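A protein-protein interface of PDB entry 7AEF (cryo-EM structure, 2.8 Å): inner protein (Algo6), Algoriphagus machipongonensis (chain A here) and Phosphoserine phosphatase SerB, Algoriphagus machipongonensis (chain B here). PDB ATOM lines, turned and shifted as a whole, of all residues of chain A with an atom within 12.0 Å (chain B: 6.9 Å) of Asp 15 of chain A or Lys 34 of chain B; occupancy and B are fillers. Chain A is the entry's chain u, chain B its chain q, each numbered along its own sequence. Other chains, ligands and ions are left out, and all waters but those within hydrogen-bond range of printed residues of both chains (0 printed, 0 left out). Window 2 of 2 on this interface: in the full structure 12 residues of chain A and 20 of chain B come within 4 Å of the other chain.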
ATOM      1  N   HIS A   9      14.588  -6.742 -12.461  1.00  0.00           N
ATOM      2  CA  HIS A   9      13.486  -5.917 -12.931  1.00  0.00           C
ATOM      3  C   HIS A   9      12.285  -6.808 -13.220  1.00  0.00           C
ATOM      4  O   HIS A   9      12.438  -7.992 -13.523  1.00  0.00           O
ATOM      5  CB  HIS A   9      13.880  -5.135 -14.194  1.00  0.00           C
ATOM      6  CG  HIS A   9      13.115  -3.863 -14.390  1.00  0.00           C
ATOM      7  ND1 HIS A   9      13.285  -2.759 -13.581  1.00  0.00           N
ATOM      8  CD2 HIS A   9      12.189  -3.514 -15.313  1.00  0.00           C
ATOM      9  CE1 HIS A   9      12.488  -1.788 -13.994  1.00  0.00           C
ATOM     10  NE2 HIS A   9      11.813  -2.220 -15.042  1.00  0.00           N
ATOM     11  N   ILE A  10      11.085  -6.227 -13.114  1.00  0.00           N
ATOM     12  CA  ILE A  10       9.866  -6.987 -13.359  1.00  0.00           C
ATOM     13  C   ILE A  10       9.720  -7.245 -14.856  1.00  0.00           C
ATOM     14  O   ILE A  10      10.078  -6.407 -15.694  1.00  0.00           O
ATOM     15  CB  ILE A  10       8.650  -6.260 -12.747  1.00  0.00           C
ATOM     16  CG1 ILE A  10       7.381  -7.120 -12.817  1.00  0.00           C
ATOM     17  CG2 ILE A  10       8.433  -4.873 -13.348  1.00  0.00           C
ATOM     18  CD1 ILE A  10       6.168  -6.518 -12.163  1.00  0.00           C
ATOM     19  N   LYS A  11       9.227  -8.433 -15.199  1.00  0.00           N
ATOM     20  CA  LYS A  11       9.173  -8.921 -16.570  1.00  0.00           C
ATOM     21  C   LYS A  11       7.805  -8.627 -17.178  1.00  0.00           C
ATOM     22  O   LYS A  11       6.786  -9.123 -16.691  1.00  0.00           O
ATOM     23  CB  LYS A  11       9.476 -10.422 -16.597  1.00  0.00           C
ATOM     24  CG  LYS A  11       9.020 -11.180 -17.828  1.00  0.00           C
ATOM     25  CD  LYS A  11       9.215 -12.668 -17.615  1.00  0.00           C
ATOM     26  CE  LYS A  11       8.375 -13.493 -18.566  1.00  0.00           C
ATOM     27  NZ  LYS A  11       8.147 -14.867 -18.041  1.00  0.00           N
ATOM     28  N   ILE A  12       7.786  -7.796 -18.220  1.00  0.00           N
ATOM     29  CA  ILE A  12       6.578  -7.469 -18.975  1.00  0.00           C
ATOM     30  C   ILE A  12       6.833  -7.809 -20.438  1.00  0.00           C
ATOM     31  O   ILE A  12       7.791  -7.305 -21.034  1.00  0.00           O
ATOM     32  CB  ILE A  12       6.185  -5.985 -18.831  1.00  0.00           C
ATOM     33  CG1 ILE A  12       6.425  -5.474 -17.406  1.00  0.00           C
ATOM     34  CG2 ILE A  12       4.741  -5.772 -19.251  1.00  0.00           C
ATOM     35  CD1 ILE A  12       6.013  -4.051 -17.177  1.00  0.00           C
ATOM     36  N   THR A  13       5.981  -8.651 -21.018  1.00  0.00           N
ATOM     37  CA  THR A  13       6.103  -9.036 -22.418  1.00  0.00           C
ATOM     38  C   THR A  13       5.007  -8.374 -23.246  1.00  0.00           C
ATOM     39  O   THR A  13       4.038  -7.830 -22.715  1.00  0.00           O
ATOM     40  CB  THR A  13       6.039 -10.560 -22.597  1.00  0.00           C
ATOM     41  OG1 THR A  13       4.675 -10.989 -22.641  1.00  0.00           O
ATOM     42  CG2 THR A  13       6.739 -11.270 -21.459  1.00  0.00           C
ATOM     43  N   VAL A  14       5.173  -8.435 -24.564  1.00  0.00           N
ATOM     44  CA  VAL A  14       4.260  -7.814 -25.518  1.00  0.00           C
ATOM     45  C   VAL A  14       3.699  -8.908 -26.420  1.00  0.00           C
ATOM     46  O   VAL A  14       4.455  -9.725 -26.955  1.00  0.00           O
ATOM     47  CB  VAL A  14       4.982  -6.718 -26.331  1.00  0.00           C
ATOM     48  CG1 VAL A  14       4.241  -6.382 -27.597  1.00  0.00           C
ATOM     49  CG2 VAL A  14       5.141  -5.462 -25.497  1.00  0.00           C
ATOM     50  N   ASP A  15       2.377  -8.928 -26.578  1.00  0.00           N
ATOM     51  CA  ASP A  15       1.708  -9.855 -27.490  1.00  0.00           C
ATOM     52  C   ASP A  15       1.679  -9.217 -28.874  1.00  0.00           C
ATOM     53  O   ASP A  15       0.687  -8.595 -29.262  1.00  0.00           O
ATOM     54  CB  ASP A  15       0.304 -10.173 -26.997  1.00  0.00           C
ATOM     55  CG  ASP A  15       0.302 -11.010 -25.739  1.00  0.00           C
ATOM     56  OD1 ASP A  15       0.055 -12.224 -25.842  1.00  0.00           O
ATOM     57  OD2 ASP A  15       0.540 -10.458 -24.646  1.00  0.00           O
ATOM     58  N   ASP A  16       2.764  -9.390 -29.631  1.00  0.00           N
ATOM     59  CA  ASP A  16       2.960  -8.711 -30.907  1.00  0.00           C
ATOM     60  C   ASP A  16       2.801  -9.641 -32.105  1.00  0.00           C
ATOM     61  O   ASP A  16       3.536  -9.510 -33.089  1.00  0.00           O
ATOM     62  CB  ASP A  16       4.332  -8.032 -30.935  1.00  0.00           C
ATOM     63  CG  ASP A  16       5.458  -8.933 -30.429  1.00  0.00           C
ATOM     64  OD1 ASP A  16       5.270 -10.164 -30.339  1.00  0.00           O
ATOM     65  OD2 ASP A  16       6.545  -8.403 -30.126  1.00  0.00           O
ATOM     66  N   SER A  17       1.853 -10.568 -32.049  1.00  0.00           N
ATOM     67  CA  SER A  17       1.690 -11.559 -33.103  1.00  0.00           C
ATOM     68  C   SER A  17       0.235 -11.998 -33.234  1.00  0.00           C
ATOM     69  O   SER A  17      -0.068 -13.009 -33.867  1.00  0.00           O
ATOM     70  CB  SER A  17       2.586 -12.772 -32.830  1.00  0.00           C
ATOM     71  OG  SER A  17       2.423 -13.772 -33.819  1.00  0.00           O
ATOM     72  N   GLU A  29       9.300 -13.090 -26.327  1.00  0.00           N
ATOM     73  CA  GLU A  29      10.130 -13.285 -25.145  1.00  0.00           C
ATOM     74  C   GLU A  29      11.571 -13.543 -25.559  1.00  0.00           C
ATOM     75  O   GLU A  29      12.410 -13.927 -24.747  1.00  0.00           O
ATOM     76  CB  GLU A  29       9.589 -14.432 -24.293  1.00  0.00           C
ATOM     77  CG  GLU A  29       8.274 -14.087 -23.609  1.00  0.00           C
ATOM     78  CD  GLU A  29       7.779 -15.177 -22.681  1.00  0.00           C
ATOM     79  OE1 GLU A  29       6.747 -15.807 -22.998  1.00  0.00           O
ATOM     80  OE2 GLU A  29       8.419 -15.401 -21.633  1.00  0.00           O
ATOM     81  N   ASP A  30      11.842 -13.341 -26.848  1.00  0.00           N
ATOM     82  CA  ASP A  30      13.223 -13.288 -27.311  1.00  0.00           C
ATOM     83  C   ASP A  30      13.868 -11.970 -26.902  1.00  0.00           C
ATOM     84  O   ASP A  30      15.054 -11.931 -26.553  1.00  0.00           O
ATOM     85  CB  ASP A  30      13.263 -13.462 -28.831  1.00  0.00           C
ATOM     86  CG  ASP A  30      14.670 -13.387 -29.403  1.00  0.00           C
ATOM     87  OD1 ASP A  30      14.804 -13.007 -30.584  1.00  0.00           O
ATOM     88  OD2 ASP A  30      15.637 -13.760 -28.703  1.00  0.00           O
ATOM     89  N   LYS A  31      13.092 -10.884 -26.915  1.00  0.00           N
ATOM     90  CA  LYS A  31      13.631  -9.573 -26.574  1.00  0.00           C
ATOM     91  C   LYS A  31      13.787  -9.411 -25.070  1.00  0.00           C
ATOM     92  O   LYS A  31      14.453  -8.481 -24.610  1.00  0.00           O
ATOM     93  CB  LYS A  31      12.727  -8.477 -27.134  1.00  0.00           C
ATOM     94  CG  LYS A  31      12.391  -8.645 -28.600  1.00  0.00           C
ATOM     95  CD  LYS A  31      11.300  -7.685 -29.021  1.00  0.00           C
ATOM     96  CE  LYS A  31      10.961  -7.842 -30.491  1.00  0.00           C
ATOM     97  NZ  LYS A  31       9.690  -7.162 -30.854  1.00  0.00           N
ATOM     98  N   GLN A  32      13.173 -10.302 -24.290  1.00  0.00           N
ATOM     99  CA  GLN A  32      13.312 -10.242 -22.838  1.00  0.00           C
ATOM    100  C   GLN A  32      14.707 -10.656 -22.403  1.00  0.00           C
ATOM    101  O   GLN A  32      15.238 -10.137 -21.416  1.00  0.00           O
ATOM    102  CB  GLN A  32      12.265 -11.140 -22.179  1.00  0.00           C
ATOM    103  CG  GLN A  32      11.759 -10.643 -20.838  1.00  0.00           C
ATOM    104  CD  GLN A  32      10.792  -9.487 -20.977  1.00  0.00           C
ATOM    105  OE1 GLN A  32      10.247  -9.241 -22.051  1.00  0.00           O
ATOM    106  NE2 GLN A  32      10.578  -8.766 -19.889  1.00  0.00           N
ATOM    107  N   HIS B  18      -3.794 -17.239  -8.301  1.00  0.00           N
ATOM    108  CA  HIS B  18      -3.547 -16.194  -7.314  1.00  0.00           C
ATOM    109  C   HIS B  18      -4.803 -15.413  -6.982  1.00  0.00           C
ATOM    110  O   HIS B  18      -5.800 -15.486  -7.702  1.00  0.00           O
ATOM    111  CB  HIS B  18      -2.480 -15.201  -7.795  1.00  0.00           C
ATOM    112  CG  HIS B  18      -2.849 -14.420  -9.010  1.00  0.00           C
ATOM    113  ND1 HIS B  18      -2.570 -14.847 -10.284  1.00  0.00           N
ATOM    114  CD2 HIS B  18      -3.502 -13.251  -9.146  1.00  0.00           C
ATOM    115  CE1 HIS B  18      -3.025 -13.965 -11.146  1.00  0.00           C
ATOM    116  NE2 HIS B  18      -3.597 -12.992 -10.482  1.00  0.00           N
ATOM    117  N   GLN B  32      -7.449  -7.623 -15.659  1.00  0.00           N
ATOM    118  CA  GLN B  32      -6.419  -8.567 -16.042  1.00  0.00           C
ATOM    119  C   GLN B  32      -5.072  -8.174 -15.509  1.00  0.00           C
ATOM    120  O   GLN B  32      -4.547  -7.100 -15.817  1.00  0.00           O
ATOM    121  CB  GLN B  32      -6.357  -8.779 -17.546  1.00  0.00           C
ATOM    122  CG  GLN B  32      -7.585  -9.447 -18.107  1.00  0.00           C
ATOM    123  CD  GLN B  32      -7.422  -9.859 -19.542  1.00  0.00           C
ATOM    124  OE1 GLN B  32      -6.357  -9.697 -20.129  1.00  0.00           O
ATOM    125  NE2 GLN B  32      -8.468 -10.411 -20.117  1.00  0.00           N
ATOM    126  N   VAL B  33      -4.524  -9.056 -14.688  1.00  0.00           N
ATOM    127  CA  VAL B  33      -3.249  -8.826 -14.059  1.00  0.00           C
ATOM    128  C   VAL B  33      -2.215  -9.587 -14.848  1.00  0.00           C
ATOM    129  O   VAL B  33      -2.275 -10.806 -14.970  1.00  0.00           O
ATOM    130  CB  VAL B  33      -3.298  -9.270 -12.589  1.00  0.00           C
ATOM    131  CG1 VAL B  33      -1.946  -9.034 -11.902  1.00  0.00           C
ATOM    132  CG2 VAL B  33      -4.406  -8.499 -11.897  1.00  0.00           C
ATOM    133  N   LYS B  34      -1.321  -8.828 -15.436  1.00  0.00           N
ATOM    134  CA  LYS B  34      -0.284  -9.284 -16.327  1.00  0.00           C
ATOM    135  C   LYS B  34       0.892  -9.842 -15.559  1.00  0.00           C
ATOM    136  O   LYS B  34       1.472 -10.856 -15.931  1.00  0.00           O
ATOM    137  CB  LYS B  34       0.094  -8.112 -17.233  1.00  0.00           C
ATOM    138  CG  LYS B  34       1.154  -8.315 -18.295  1.00  0.00           C
ATOM    139  CD  LYS B  34       0.757  -9.308 -19.365  1.00  0.00           C
ATOM    140  CE  LYS B  34       1.694  -9.193 -20.569  1.00  0.00           C
ATOM    141  NZ  LYS B  34       1.559 -10.329 -21.547  1.00  0.00           N
ATOM    142  N   SER B  35       1.260  -9.175 -14.475  1.00  0.00           N
ATOM    143  CA  SER B  35       2.441  -9.606 -13.720  1.00  0.00           C
ATOM    144  C   SER B  35       2.452  -9.214 -12.244  1.00  0.00           C
ATOM    145  O   SER B  35       1.929  -8.160 -11.857  1.00  0.00           O
ATOM    146  CB  SER B  35       3.681  -9.068 -14.387  1.00  0.00           C
ATOM    147  OG  SER B  35       4.817  -9.454 -13.695  1.00  0.00           O
ATOM    148  N   ILE B  36       2.993 -10.112 -11.395  1.00  0.00           N
ATOM    149  CA  ILE B  36       3.143  -9.858  -9.954  1.00  0.00           C
ATOM    150  C   ILE B  36       4.582 -10.049  -9.446  1.00  0.00           C
ATOM    151  O   ILE B  36       5.211 -11.079  -9.688  1.00  0.00           O
ATOM    152  CB  ILE B  36       2.224 -10.780  -9.113  1.00  0.00           C
ATOM    153  CG1 ILE B  36       0.769 -10.564  -9.512  1.00  0.00           C
ATOM    154  CG2 ILE B  36       2.442 -10.515  -7.583  1.00  0.00           C
ATOM    155  CD1 ILE B  36      -0.202 -11.540  -8.931  1.00  0.00           C
ATOM    156  N   LEU B  50       2.180  -4.650  -8.926  1.00  0.00           N
ATOM    157  CA  LEU B  50       1.189  -5.273  -9.803  1.00  0.00           C
ATOM    158  C   LEU B  50       1.111  -4.576 -11.153  1.00  0.00           C
ATOM    159  O   LEU B  50       1.037  -3.349 -11.222  1.00  0.00           O
ATOM    160  CB  LEU B  50      -0.218  -5.187  -9.193  1.00  0.00           C
ATOM    161  CG  LEU B  50      -0.460  -5.790  -7.805  1.00  0.00           C
ATOM    162  CD1 LEU B  50      -1.880  -5.454  -7.379  1.00  0.00           C
ATOM    163  CD2 LEU B  50      -0.247  -7.276  -7.829  1.00  0.00           C
ATOM    164  N   VAL B  51       1.067  -5.351 -12.232  1.00  0.00           N
ATOM    165  CA  VAL B  51       0.886  -4.765 -13.559  1.00  0.00           C
ATOM    166  C   VAL B  51      -0.470  -5.183 -14.105  1.00  0.00           C
ATOM    167  O   VAL B  51      -0.721  -6.377 -14.307  1.00  0.00           O
ATOM    168  CB  VAL B  51       1.992  -5.199 -14.536  1.00  0.00           C
ATOM    169  CG1 VAL B  51       1.753  -4.564 -15.898  1.00  0.00           C
ATOM    170  CG2 VAL B  51       3.342  -4.813 -13.982  1.00  0.00           C
ATOM    171  N   ILE B  52      -1.313  -4.183 -14.363  1.00  0.00           N
ATOM    172  CA  ILE B  52      -2.699  -4.330 -14.800  1.00  0.00           C
ATOM    173  C   ILE B  52      -2.912  -3.730 -16.192  1.00  0.00           C
ATOM    174  O   ILE B  52      -2.467  -2.621 -16.477  1.00  0.00           O
ATOM    175  CB  ILE B  52      -3.634  -3.644 -13.779  1.00  0.00           C
ATOM    176  CG1 ILE B  52      -3.440  -4.290 -12.394  1.00  0.00           C
ATOM    177  CG2 ILE B  52      -5.098  -3.780 -14.228  1.00  0.00           C
ATOM    178  CD1 ILE B  52      -4.051  -3.537 -11.255  1.00  0.00           C
ATOM    179  N   LEU B  53      -3.560  -4.460 -17.086  1.00  0.00           N
ATOM    180  CA  LEU B  53      -3.763  -3.919 -18.432  1.00  0.00           C
ATOM    181  C   LEU B  53      -4.878  -2.883 -18.400  1.00  0.00           C
ATOM    182  O   LEU B  53      -5.936  -3.156 -17.842  1.00  0.00           O
ATOM    183  CB  LEU B  53      -4.155  -5.042 -19.385  1.00  0.00           C
ATOM    184  CG  LEU B  53      -3.152  -6.207 -19.536  1.00  0.00           C
ATOM    185  CD1 LEU B  53      -3.754  -7.238 -20.432  1.00  0.00           C
ATOM    186  CD2 LEU B  53      -1.822  -5.720 -20.078  1.00  0.00           C
ATOM    187  N   ASN B 104       1.917   0.908 -29.155  1.00  0.00           N
ATOM    188  CA  ASN B 104       0.971  -0.193 -29.166  1.00  0.00           C
ATOM    189  C   ASN B 104       0.853  -0.829 -27.781  1.00  0.00           C
ATOM    190  O   ASN B 104       0.729  -2.048 -27.660  1.00  0.00           O
ATOM    191  CB  ASN B 104       1.346  -1.204 -30.224  1.00  0.00           C
ATOM    192  CG  ASN B 104       0.204  -2.109 -30.619  1.00  0.00           C
ATOM    193  OD1 ASN B 104      -0.958  -1.706 -30.636  1.00  0.00           O
ATOM    194  ND2 ASN B 104       0.520  -3.327 -30.955  1.00  0.00           N
ATOM    195  N   GLN B 105       0.928  -0.013 -26.730  1.00  0.00           N
ATOM    196  CA  GLN B 105       0.841  -0.522 -25.361  1.00  0.00           C
ATOM    197  C   GLN B 105       0.258   0.474 -24.369  1.00  0.00           C
ATOM    198  O   GLN B 105       0.603   1.653 -24.374  1.00  0.00           O
ATOM    199  CB  GLN B 105       2.217  -0.964 -24.866  1.00  0.00           C
ATOM    200  CG  GLN B 105       2.223  -1.553 -23.474  1.00  0.00           C
ATOM    201  CD  GLN B 105       3.563  -2.025 -23.053  1.00  0.00           C
ATOM    202  OE1 GLN B 105       4.544  -1.277 -23.046  1.00  0.00           O
ATOM    203  NE2 GLN B 105       3.635  -3.291 -22.690  1.00  0.00           N
ATOM    204  N   ILE B 107      -0.622   0.438 -20.070  1.00  0.00           N
ATOM    205  CA  ILE B 107      -0.719  -0.269 -18.787  1.00  0.00           C
ATOM    206  C   ILE B 107      -0.815   0.626 -17.546  1.00  0.00           C
ATOM    207  O   ILE B 107      -0.421   1.796 -17.553  1.00  0.00           O
ATOM    208  CB  ILE B 107       0.466  -1.240 -18.581  1.00  0.00           C
ATOM    209  CG1 ILE B 107       1.783  -0.467 -18.521  1.00  0.00           C
ATOM    210  CG2 ILE B 107       0.486  -2.284 -19.694  1.00  0.00           C
ATOM    211  CD1 ILE B 107       2.959  -1.288 -18.112  1.00  0.00           C
ATOM    212  N   ILE B 337       5.928 -13.839 -10.568  1.00  0.00           N
ATOM    213  CA  ILE B 337       4.839 -14.629 -11.123  1.00  0.00           C
ATOM    214  C   ILE B 337       4.339 -14.049 -12.436  1.00  0.00           C
ATOM    215  O   ILE B 337       3.803 -12.938 -12.490  1.00  0.00           O
ATOM    216  CB  ILE B 337       3.667 -14.716 -10.129  1.00  0.00           C
ATOM    217  CG1 ILE B 337       4.144 -15.267  -8.812  1.00  0.00           C
ATOM    218  CG2 ILE B 337       2.562 -15.589 -10.665  1.00  0.00           C
ATOM    219  CD1 ILE B 337       4.449 -14.209  -7.748  1.00  0.00           C
ATOM    220  N   SER B 338       4.530 -14.797 -13.518  1.00  0.00           N
ATOM    221  CA  SER B 338       4.103 -14.337 -14.840  1.00  0.00           C
ATOM    222  C   SER B 338       4.146 -15.416 -15.906  1.00  0.00           C
ATOM    223  O   SER B 338       4.916 -16.373 -15.819  1.00  0.00           O
ATOM    224  CB  SER B 338       4.948 -13.170 -15.325  1.00  0.00           C
ATOM    225  OG  SER B 338       6.271 -13.556 -15.569  1.00  0.00           O
ATOM    226  N   GLU B 339       3.331 -15.235 -16.941  1.00  0.00           N
ATOM    227  CA  GLU B 339       3.315 -16.066 -18.141  1.00  0.00           C
ATOM    228  C   GLU B 339       3.305 -17.563 -17.875  1.00  0.00           C
ATOM    229  O   GLU B 339       4.007 -18.322 -18.539  1.00  0.00           O
ATOM    230  CB  GLU B 339       4.474 -15.697 -19.060  1.00  0.00           C
ATOM    231  CG  GLU B 339       4.468 -14.221 -19.520  1.00  0.00           C
ATOM    232  CD  GLU B 339       3.293 -13.827 -20.449  1.00  0.00           C
ATOM    233  OE1 GLU B 339       2.713 -14.684 -21.055  1.00  0.00           O
ATOM    234  OE2 GLU B 339       2.990 -12.645 -20.521  1.00  0.00           O
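The side-chain amino group of Lys 11 of chain A lies within salt-bridge range of the side-chain carboxylate of Glu 29 of chain A (3.6 Å).
The backbone NH (N) of Lys 34 of chain B lies within hydrogen-bond range of the backbone carbonyl oxygen (O) of Val 51 of chain B (2.8 Å).
The side-chain carboxylate of Glu 339 of chain B lies within salt-bridge range of the side-chain amino group of Lys 34 of chain B.
The backbone carbonyl oxygen (O) of Ser 35 of chain B sits at hydrogen-bond distance from the backbone NH (N) of Val 51 of chain B, at 3.0 Å.
Of chain B, only Lys 34 (3.3 Å) comes within 4 Å of Asp 15 of chain A.
Of chain A, only Thr 13 and Asp 15 come within 4 Å of Lys 34 of chain B.
No residue of chain A comes within 4 Å of Val 33 of chain B.
Of chain A, only Ile 10 (3.6 Å) and Lys 11 (3.6 Å) come within 4 Å of Ser 35 of chain B.
Val 51 of chain B touches just one residue of chain A: Ile 10 (3.8 Å).
No residue of chain A comes within 4 Å of Leu 53 of chain B.
Ser 338 of chain B touches one residue of chain A.
Printed residues of chain B within 4 Å of Lys 11 of chain A: Ser 35, Ser 338 and Glu 339.
Of the printed residues of chain A, Gln 105 of chain B touches Val 14 (3.9 Å).
Printed residues of chain B within 4 Å of Val 14 of chain A: Gln 105.
Printed residues of chain A within 4 Å of Glu 339 of chain B: Lys 11 (3.9 Å) and Thr 13 (3.2 Å).
Of the printed residues of chain B, Ile 10 of chain A touches Ser 35 and Val 51.
Asn 104 of chain B touches none of the printed residues of chain A.
The nearest residue of chain B that does not touch Asp 15 of chain A is Glu 339 of chain B (5.3 Å).
The nearest residue of chain A that does not touch Lys 34 of chain B is Ile 12 of chain A (4.5 Å).
Printed residues of chain A that touch a printed residue of chain B: Ile 10, Lys 11, Thr 13, Val 14 and Asp 15.
Hydrophobic or aromatic side chains of chain A that line the printed part of chain B: Ile 10 and Val 14.
Hydrophobic or aromatic side chains of chain B within 4 Å of the printed part of chain A: Val 51.
The side-chain amino group of Lys 11 of chain A lies within hydrogen-bond range of the side-chain hydroxyl of Ser 338 of chain B.
The side-chain amino group (NZ) of Lys 34 of chain B lies within hydrogen-bond range of the side-chain hydroxyl (OG1) of Thr 13 of chain A.
OG1 of Thr 13 of chain A lies within hydrogen-bond range of OE2 of Glu 339 of chain B (3.2 Å).
The side-chain carboxylate (OD2) of Asp 15 of chain A lies within salt-bridge range of the side-chain amino group (NZ) of Lys 34 of chain B, 3.3 Å away.
Ile 10 of chain A touches Ser 35 of chain B.
Val 51 of chain B touches Ile 10 of chain A (CG2 to CD1, 3.8 Å).
Lys 11 of chain A touches Ser 35 of chain B (O to OG, 3.6 Å).
CB of Glu 339 of chain B touches NZ of Lys 11 of chain A, 3.9 Å away.
CG2 of Val 14 of chain A touches NE2 of Gln 105 of chain B (3.9 Å).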
